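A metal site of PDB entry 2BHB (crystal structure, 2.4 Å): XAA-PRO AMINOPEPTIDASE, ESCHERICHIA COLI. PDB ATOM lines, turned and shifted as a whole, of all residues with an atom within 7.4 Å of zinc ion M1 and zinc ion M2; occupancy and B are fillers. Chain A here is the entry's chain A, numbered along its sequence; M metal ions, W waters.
OD2 of Asp 260 sits close to OG1 of Thr 273. The side-chain carboxylate (OD1) of Asp 260 sits close to the side-chain hydroxyl (OH) of Tyr 229, at 2.7 Å. The backbone carbonyl oxygen (O) of Asp 260 sits at hydrogen-bond distance from the backbone NH (N) of Ile 232 (2.9 Å). The backbone NH (N) of Glu 406 sits at hydrogen-bond distance from the backbone carbonyl oxygen (O) of Thr 273 (3.0 Å). OD1 of Asp 271 lies close to OH of Tyr 229. The backbone NH (N) of Asp 271 is in hydrogen-bond range of the side-chain carboxylate (OD2) of Asp 408, at 2.9 Å. ND1 of His 354 sits close to O of Val 360, at 2.9 Å. OG1 of Thr 381 lies close to OE2 of Glu 383 (2.7 Å).
OH of Tyr 229 touches zinc ion M1, 3.7 Å away. Thr 273 touches zinc ion M1. Five residues have an atom within 4 Å of zinc ion M1: Tyr 229, Asp 260, Asp 271, Thr 273 and Glu 406.
Residues that only touch zinc ion M2: Thr 381. Five residues have an atom within 4 Å of zinc ion M2: Asp 271, His 354, Thr 381, Glu 383 and Glu 406. The nearest printed residue that does not touch zinc ion M2 is His 361 (4.6 Å).
Zinc ion M1 is bound by water W1, 1.9 Å away. Zinc ion M1 is bound by OD1 of Asp 260, 2.1 Å away. OE1 of Glu 406 is bound to zinc ion M1 (2.1 Å). OD1 of Asp 271 is bound to zinc ion M1 (2.1 Å). The side-chain carboxylate (OD2) of Asp 260 binds zinc ion M1 (2.6 Å). Zinc ion M1 has five donor atoms within binding distance.
Zinc ion M2 is bound by water W1 (2.1 Å), a ring nitrogen (NE2) of His 354 (2.1 Å), the side-chain carboxylate of Glu 406 (2.1 Å), the side-chain carboxylate of Asp 271 (2.2 Å) and the side-chain carboxylate of Glu 383 (2.4 Å).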
ATOM      1  N   TYR A 229      20.172 -14.945  -9.109  1.00  0.00           N
ATOM      2  CA  TYR A 229      19.620 -13.640  -9.460  1.00  0.00           C
ATOM      3  C   TYR A 229      18.856 -13.093  -8.255  1.00  0.00           C
ATOM      4  O   TYR A 229      18.530 -13.837  -7.338  1.00  0.00           O
ATOM      5  CB  TYR A 229      18.712 -13.738 -10.708  1.00  0.00           C
ATOM      6  CG  TYR A 229      17.602 -14.748 -10.555  1.00  0.00           C
ATOM      7  CD1 TYR A 229      17.844 -16.096 -10.759  1.00  0.00           C
ATOM      8  CD2 TYR A 229      16.322 -14.360 -10.167  1.00  0.00           C
ATOM      9  CE1 TYR A 229      16.840 -17.036 -10.586  1.00  0.00           C
ATOM     10  CE2 TYR A 229      15.301 -15.305 -10.011  1.00  0.00           C
ATOM     11  CZ  TYR A 229      15.586 -16.636 -10.222  1.00  0.00           C
ATOM     12  OH  TYR A 229      14.604 -17.594 -10.059  1.00  0.00           O
ATOM     13  N   ILE A 232      12.548 -12.456  -6.389  1.00  0.00           N
ATOM     14  CA  ILE A 232      11.313 -11.717  -6.619  1.00  0.00           C
ATOM     15  C   ILE A 232      10.215 -12.290  -5.726  1.00  0.00           C
ATOM     16  O   ILE A 232       9.897 -13.463  -5.836  1.00  0.00           O
ATOM     17  CB  ILE A 232      10.897 -11.821  -8.113  1.00  0.00           C
ATOM     18  CG1 ILE A 232      11.890 -11.032  -8.997  1.00  0.00           C
ATOM     19  CG2 ILE A 232       9.460 -11.320  -8.353  1.00  0.00           C
ATOM     20  CD1 ILE A 232      12.072 -11.616 -10.366  1.00  0.00           C
ATOM     21  N   ILE A 259       6.597 -15.850  -6.400  1.00  0.00           N
ATOM     22  CA  ILE A 259       8.004 -15.967  -6.017  1.00  0.00           C
ATOM     23  C   ILE A 259       8.807 -16.516  -7.184  1.00  0.00           C
ATOM     24  O   ILE A 259       8.568 -17.640  -7.631  1.00  0.00           O
ATOM     25  CB  ILE A 259       8.182 -16.877  -4.791  1.00  0.00           C
ATOM     26  CG1 ILE A 259       7.293 -16.383  -3.651  1.00  0.00           C
ATOM     27  CG2 ILE A 259       9.659 -16.933  -4.390  1.00  0.00           C
ATOM     28  CD1 ILE A 259       7.551 -17.064  -2.309  1.00  0.00           C
ATOM     29  N   ASP A 260       9.738 -15.707  -7.693  1.00  0.00           N
ATOM     30  CA  ASP A 260      10.732 -16.128  -8.683  1.00  0.00           C
ATOM     31  C   ASP A 260      12.106 -16.099  -7.999  1.00  0.00           C
ATOM     32  O   ASP A 260      12.631 -15.034  -7.667  1.00  0.00           O
ATOM     33  CB  ASP A 260      10.718 -15.211  -9.910  1.00  0.00           C
ATOM     34  CG  ASP A 260      11.340 -15.869 -11.164  1.00  0.00           C
ATOM     35  OD1 ASP A 260      12.186 -16.794 -11.073  1.00  0.00           O
ATOM     36  OD2 ASP A 260      10.969 -15.440 -12.270  1.00  0.00           O
ATOM     37  N   ALA A 261      12.650 -17.287  -7.769  1.00  0.00           N
ATOM     38  CA  ALA A 261      13.875 -17.416  -7.000  1.00  0.00           C
ATOM     39  C   ALA A 261      14.628 -18.681  -7.403  1.00  0.00           C
ATOM     40  O   ALA A 261      14.034 -19.712  -7.736  1.00  0.00           O
ATOM     41  CB  ALA A 261      13.572 -17.434  -5.504  1.00  0.00           C
ATOM     42  N   GLY A 262      15.959 -18.579  -7.371  1.00  0.00           N
ATOM     43  CA  GLY A 262      16.836 -19.624  -7.837  1.00  0.00           C
ATOM     44  C   GLY A 262      18.180 -19.521  -7.156  1.00  0.00           C
ATOM     45  O   GLY A 262      18.687 -18.421  -6.934  1.00  0.00           O
ATOM     46  N   GLY A 270      19.590 -22.535 -10.531  1.00  0.00           N
ATOM     47  CA  GLY A 270      18.206 -22.944 -10.446  1.00  0.00           C
ATOM     48  C   GLY A 270      17.367 -21.720 -10.759  1.00  0.00           C
ATOM     49  O   GLY A 270      17.838 -20.599 -10.643  1.00  0.00           O
ATOM     50  N   ASP A 271      16.123 -21.935 -11.162  1.00  0.00           N
ATOM     51  CA  ASP A 271      15.245 -20.837 -11.557  1.00  0.00           C
ATOM     52  C   ASP A 271      13.789 -21.296 -11.527  1.00  0.00           C
ATOM     53  O   ASP A 271      13.282 -21.865 -12.512  1.00  0.00           O
ATOM     54  CB  ASP A 271      15.640 -20.330 -12.944  1.00  0.00           C
ATOM     55  CG  ASP A 271      14.818 -19.146 -13.374  1.00  0.00           C
ATOM     56  OD1 ASP A 271      14.032 -18.643 -12.552  1.00  0.00           O
ATOM     57  OD2 ASP A 271      14.965 -18.717 -14.531  1.00  0.00           O
ATOM     58  N   ILE A 272      13.115 -21.078 -10.406  1.00  0.00           N
ATOM     59  CA  ILE A 272      11.731 -21.516 -10.241  1.00  0.00           C
ATOM     60  C   ILE A 272      10.818 -20.315  -9.935  1.00  0.00           C
ATOM     61  O   ILE A 272      11.214 -19.377  -9.241  1.00  0.00           O
ATOM     62  CB  ILE A 272      11.613 -22.581  -9.109  1.00  0.00           C
ATOM     63  CG1 ILE A 272      12.327 -23.863  -9.492  1.00  0.00           C
ATOM     64  CG2 ILE A 272      10.133 -22.897  -8.773  1.00  0.00           C
ATOM     65  CD1 ILE A 272      12.313 -24.911  -8.398  1.00  0.00           C
ATOM     66  N   THR A 273       9.601 -20.363 -10.476  1.00  0.00           N
ATOM     67  CA  THR A 273       8.536 -19.456 -10.053  1.00  0.00           C
ATOM     68  C   THR A 273       7.362 -20.277  -9.575  1.00  0.00           C
ATOM     69  O   THR A 273       6.925 -21.211 -10.254  1.00  0.00           O
ATOM     70  CB  THR A 273       8.020 -18.489 -11.153  1.00  0.00           C
ATOM     71  OG1 THR A 273       9.118 -17.891 -11.854  1.00  0.00           O
ATOM     72  CG2 THR A 273       7.190 -17.361 -10.507  1.00  0.00           C
ATOM     73  N   LEU A 352       8.465 -17.445 -23.250  1.00  0.00           N
ATOM     74  CA  LEU A 352       8.090 -18.642 -22.506  1.00  0.00           C
ATOM     75  C   LEU A 352       9.304 -19.342 -21.877  1.00  0.00           C
ATOM     76  O   LEU A 352       9.191 -20.019 -20.851  1.00  0.00           O
ATOM     77  CB  LEU A 352       7.404 -19.624 -23.453  1.00  0.00           C
ATOM     78  CG  LEU A 352       6.845 -20.919 -22.855  1.00  0.00           C
ATOM     79  CD1 LEU A 352       5.762 -20.605 -21.851  1.00  0.00           C
ATOM     80  CD2 LEU A 352       6.331 -21.816 -23.964  1.00  0.00           C
ATOM     81  N   SER A 353      10.458 -19.206 -22.512  1.00  0.00           N
ATOM     82  CA  SER A 353      11.600 -20.048 -22.205  1.00  0.00           C
ATOM     83  C   SER A 353      12.902 -19.330 -22.461  1.00  0.00           C
ATOM     84  O   SER A 353      13.059 -18.700 -23.494  1.00  0.00           O
ATOM     85  CB  SER A 353      11.565 -21.327 -23.056  1.00  0.00           C
ATOM     86  OG  SER A 353      10.475 -22.159 -22.718  1.00  0.00           O
ATOM     87  N   HIS A 354      13.851 -19.434 -21.524  1.00  0.00           N
ATOM     88  CA  HIS A 354      15.213 -19.032 -21.791  1.00  0.00           C
ATOM     89  C   HIS A 354      16.172 -20.182 -21.485  1.00  0.00           C
ATOM     90  O   HIS A 354      15.855 -21.069 -20.692  1.00  0.00           O
ATOM     91  CB  HIS A 354      15.600 -17.750 -21.026  1.00  0.00           C
ATOM     92  CG  HIS A 354      15.434 -17.847 -19.538  1.00  0.00           C
ATOM     93  ND1 HIS A 354      16.375 -18.460 -18.728  1.00  0.00           N
ATOM     94  CD2 HIS A 354      14.457 -17.405 -18.719  1.00  0.00           C
ATOM     95  CE1 HIS A 354      15.956 -18.390 -17.468  1.00  0.00           C
ATOM     96  NE2 HIS A 354      14.810 -17.750 -17.438  1.00  0.00           N
ATOM     97  N   TRP A 355      17.328 -20.163 -22.133  1.00  0.00           N
ATOM     98  CA  TRP A 355      18.408 -21.101 -21.835  1.00  0.00           C
ATOM     99  C   TRP A 355      18.822 -20.933 -20.363  1.00  0.00           C
ATOM    100  O   TRP A 355      18.793 -19.830 -19.825  1.00  0.00           O
ATOM    101  CB  TRP A 355      19.638 -20.859 -22.707  1.00  0.00           C
ATOM    102  CG  TRP A 355      19.457 -20.833 -24.193  1.00  0.00           C
ATOM    103  CD1 TRP A 355      19.946 -19.890 -25.045  1.00  0.00           C
ATOM    104  CD2 TRP A 355      18.786 -21.806 -25.015  1.00  0.00           C
ATOM    105  NE1 TRP A 355      19.621 -20.201 -26.338  1.00  0.00           N
ATOM    106  CE2 TRP A 355      18.902 -21.371 -26.350  1.00  0.00           C
ATOM    107  CE3 TRP A 355      18.092 -22.988 -24.742  1.00  0.00           C
ATOM    108  CZ2 TRP A 355      18.349 -22.084 -27.417  1.00  0.00           C
ATOM    109  CZ3 TRP A 355      17.561 -23.709 -25.810  1.00  0.00           C
ATOM    110  CH2 TRP A 355      17.683 -23.244 -27.136  1.00  0.00           C
ATOM    111  N   LEU A 356      19.252 -22.018 -19.737  1.00  0.00           N
ATOM    112  CA  LEU A 356      19.637 -22.001 -18.339  1.00  0.00           C
ATOM    113  C   LEU A 356      20.995 -22.709 -18.152  1.00  0.00           C
ATOM    114  O   LEU A 356      21.246 -23.763 -18.739  1.00  0.00           O
ATOM    115  CB  LEU A 356      18.545 -22.672 -17.504  1.00  0.00           C
ATOM    116  CG  LEU A 356      18.734 -22.775 -15.991  1.00  0.00           C
ATOM    117  CD1 LEU A 356      18.597 -21.420 -15.309  1.00  0.00           C
ATOM    118  CD2 LEU A 356      17.730 -23.779 -15.414  1.00  0.00           C
ATOM    119  N   VAL A 360      21.659 -17.547 -15.348  1.00  0.00           N
ATOM    120  CA  VAL A 360      20.242 -17.882 -15.289  1.00  0.00           C
ATOM    121  C   VAL A 360      19.576 -17.632 -16.659  1.00  0.00           C
ATOM    122  O   VAL A 360      18.844 -18.491 -17.142  1.00  0.00           O
ATOM    123  CB  VAL A 360      19.496 -17.172 -14.104  1.00  0.00           C
ATOM    124  CG1 VAL A 360      19.549 -15.648 -14.235  1.00  0.00           C
ATOM    125  CG2 VAL A 360      18.064 -17.649 -14.039  1.00  0.00           C
ATOM    126  N   HIS A 361      19.848 -16.492 -17.271  1.00  0.00           N
ATOM    127  CA  HIS A 361      19.530 -16.258 -18.683  1.00  0.00           C
ATOM    128  C   HIS A 361      20.776 -16.601 -19.464  1.00  0.00           C
ATOM    129  O   HIS A 361      21.647 -15.744 -19.710  1.00  0.00           O
ATOM    130  CB  HIS A 361      19.086 -14.819 -18.948  1.00  0.00           C
ATOM    131  CG  HIS A 361      17.789 -14.451 -18.290  1.00  0.00           C
ATOM    132  ND1 HIS A 361      17.367 -13.148 -18.151  1.00  0.00           N
ATOM    133  CD2 HIS A 361      16.852 -15.213 -17.682  1.00  0.00           C
ATOM    134  CE1 HIS A 361      16.216 -13.126 -17.509  1.00  0.00           C
ATOM    135  NE2 HIS A 361      15.877 -14.367 -17.224  1.00  0.00           N
ATOM    136  N   LEU A 380      16.608 -25.438 -20.378  1.00  0.00           N
ATOM    137  CA  LEU A 380      15.780 -24.255 -20.494  1.00  0.00           C
ATOM    138  C   LEU A 380      14.642 -24.197 -19.480  1.00  0.00           C
ATOM    139  O   LEU A 380      14.294 -25.194 -18.824  1.00  0.00           O
ATOM    140  CB  LEU A 380      15.209 -24.135 -21.913  1.00  0.00           C
ATOM    141  CG  LEU A 380      14.306 -25.255 -22.466  1.00  0.00           C
ATOM    142  CD1 LEU A 380      13.448 -24.699 -23.572  1.00  0.00           C
ATOM    143  CD2 LEU A 380      15.113 -26.445 -22.958  1.00  0.00           C
ATOM    144  N   THR A 381      14.082 -23.006 -19.347  1.00  0.00           N
ATOM    145  CA  THR A 381      12.957 -22.776 -18.487  1.00  0.00           C
ATOM    146  C   THR A 381      11.649 -22.841 -19.291  1.00  0.00           C
ATOM    147  O   THR A 381      11.643 -22.720 -20.514  1.00  0.00           O
ATOM    148  CB  THR A 381      13.063 -21.420 -17.783  1.00  0.00           C
ATOM    149  OG1 THR A 381      12.867 -20.359 -18.736  1.00  0.00           O
ATOM    150  CG2 THR A 381      14.435 -21.285 -17.118  1.00  0.00           C
ATOM    151  N   VAL A 382      10.557 -23.070 -18.561  1.00  0.00           N
ATOM    152  CA  VAL A 382       9.216 -23.012 -19.104  1.00  0.00           C
ATOM    153  C   VAL A 382       8.465 -22.177 -18.094  1.00  0.00           C
ATOM    154  O   VAL A 382       8.260 -22.619 -16.969  1.00  0.00           O
ATOM    155  CB  VAL A 382       8.585 -24.427 -19.236  1.00  0.00           C
ATOM    156  CG1 VAL A 382       7.313 -24.378 -20.088  1.00  0.00           C
ATOM    157  CG2 VAL A 382       9.581 -25.421 -19.847  1.00  0.00           C
ATOM    158  N   GLU A 383       8.095 -20.958 -18.477  1.00  0.00           N
ATOM    159  CA  GLU A 383       7.543 -20.004 -17.537  1.00  0.00           C
ATOM    160  C   GLU A 383       6.432 -19.126 -18.111  1.00  0.00           C
ATOM    161  O   GLU A 383       6.583 -17.900 -18.197  1.00  0.00           O
ATOM    162  CB  GLU A 383       8.674 -19.132 -16.960  1.00  0.00           C
ATOM    163  CG  GLU A 383       9.497 -18.361 -17.964  1.00  0.00           C
ATOM    164  CD  GLU A 383      10.675 -17.694 -17.313  1.00  0.00           C
ATOM    165  OE1 GLU A 383      10.459 -16.784 -16.459  1.00  0.00           O
ATOM    166  OE2 GLU A 383      11.816 -18.096 -17.635  1.00  0.00           O
ATOM    167  N   ARG A 404       2.825 -16.355 -12.465  1.00  0.00           N
ATOM    168  CA  ARG A 404       3.813 -17.066 -13.279  1.00  0.00           C
ATOM    169  C   ARG A 404       4.091 -18.394 -12.598  1.00  0.00           C
ATOM    170  O   ARG A 404       4.119 -18.480 -11.372  1.00  0.00           O
ATOM    171  CB  ARG A 404       5.102 -16.235 -13.449  1.00  0.00           C
ATOM    172  CG  ARG A 404       6.229 -16.919 -14.244  1.00  0.00           C
ATOM    173  CD  ARG A 404       7.300 -15.936 -14.757  1.00  0.00           C
ATOM    174  NE  ARG A 404       8.097 -15.234 -13.731  1.00  0.00           N
ATOM    175  CZ  ARG A 404       7.921 -13.978 -13.310  1.00  0.00           C
ATOM    176  NH1 ARG A 404       6.941 -13.206 -13.769  1.00  0.00           N
ATOM    177  NH2 ARG A 404       8.729 -13.473 -12.400  1.00  0.00           N
ATOM    178  N   GLU A 406       6.879 -21.605 -13.187  1.00  0.00           N
ATOM    179  CA  GLU A 406       8.102 -21.887 -13.922  1.00  0.00           C
ATOM    180  C   GLU A 406       8.861 -23.111 -13.435  1.00  0.00           C
ATOM    181  O   GLU A 406       9.126 -23.258 -12.244  1.00  0.00           O
ATOM    182  CB  GLU A 406       9.033 -20.673 -13.864  1.00  0.00           C
ATOM    183  CG  GLU A 406      10.467 -20.967 -14.293  1.00  0.00           C
ATOM    184  CD  GLU A 406      11.307 -19.733 -14.297  1.00  0.00           C
ATOM    185  OE1 GLU A 406      11.061 -18.844 -13.441  1.00  0.00           O
ATOM    186  OE2 GLU A 406      12.226 -19.659 -15.138  1.00  0.00           O
ATOM    187  N   ASP A 407       9.198 -23.970 -14.391  1.00  0.00           N
ATOM    188  CA  ASP A 407       9.992 -25.160 -14.156  1.00  0.00           C
ATOM    189  C   ASP A 407      11.244 -25.085 -15.047  1.00  0.00           C
ATOM    190  O   ASP A 407      11.269 -24.377 -16.060  1.00  0.00           O
ATOM    191  CB  ASP A 407       9.157 -26.424 -14.484  1.00  0.00           C
ATOM    192  CG  ASP A 407       8.361 -26.955 -13.267  1.00  0.00           C
ATOM    193  OD1 ASP A 407       8.694 -26.629 -12.105  1.00  0.00           O
ATOM    194  OD2 ASP A 407       7.408 -27.743 -13.470  1.00  0.00           O
ATOM    195  N   ASP A 408      12.287 -25.806 -14.636  1.00  0.00           N
ATOM    196  CA  ASP A 408      13.555 -25.913 -15.393  1.00  0.00           C
ATOM    197  C   ASP A 408      13.674 -27.323 -15.975  1.00  0.00           C
ATOM    198  O   ASP A 408      13.477 -28.317 -15.269  1.00  0.00           O
ATOM    199  CB  ASP A 408      14.767 -25.664 -14.472  1.00  0.00           C
ATOM    200  CG  ASP A 408      14.693 -24.340 -13.749  1.00  0.00           C
ATOM    201  OD1 ASP A 408      14.100 -23.365 -14.302  1.00  0.00           O
ATOM    202  OD2 ASP A 408      15.247 -24.271 -12.629  1.00  0.00           O
HETATM  203 ZN    ZN M   1      12.456 -17.390 -13.016  1.00  0.00          ZN
HETATM  204 ZN    ZN M   2      13.395 -18.017 -15.883  1.00  0.00          ZN
HETATM  205  O   HOH W   1      12.717 -16.473 -14.666  1.00  0.00           O
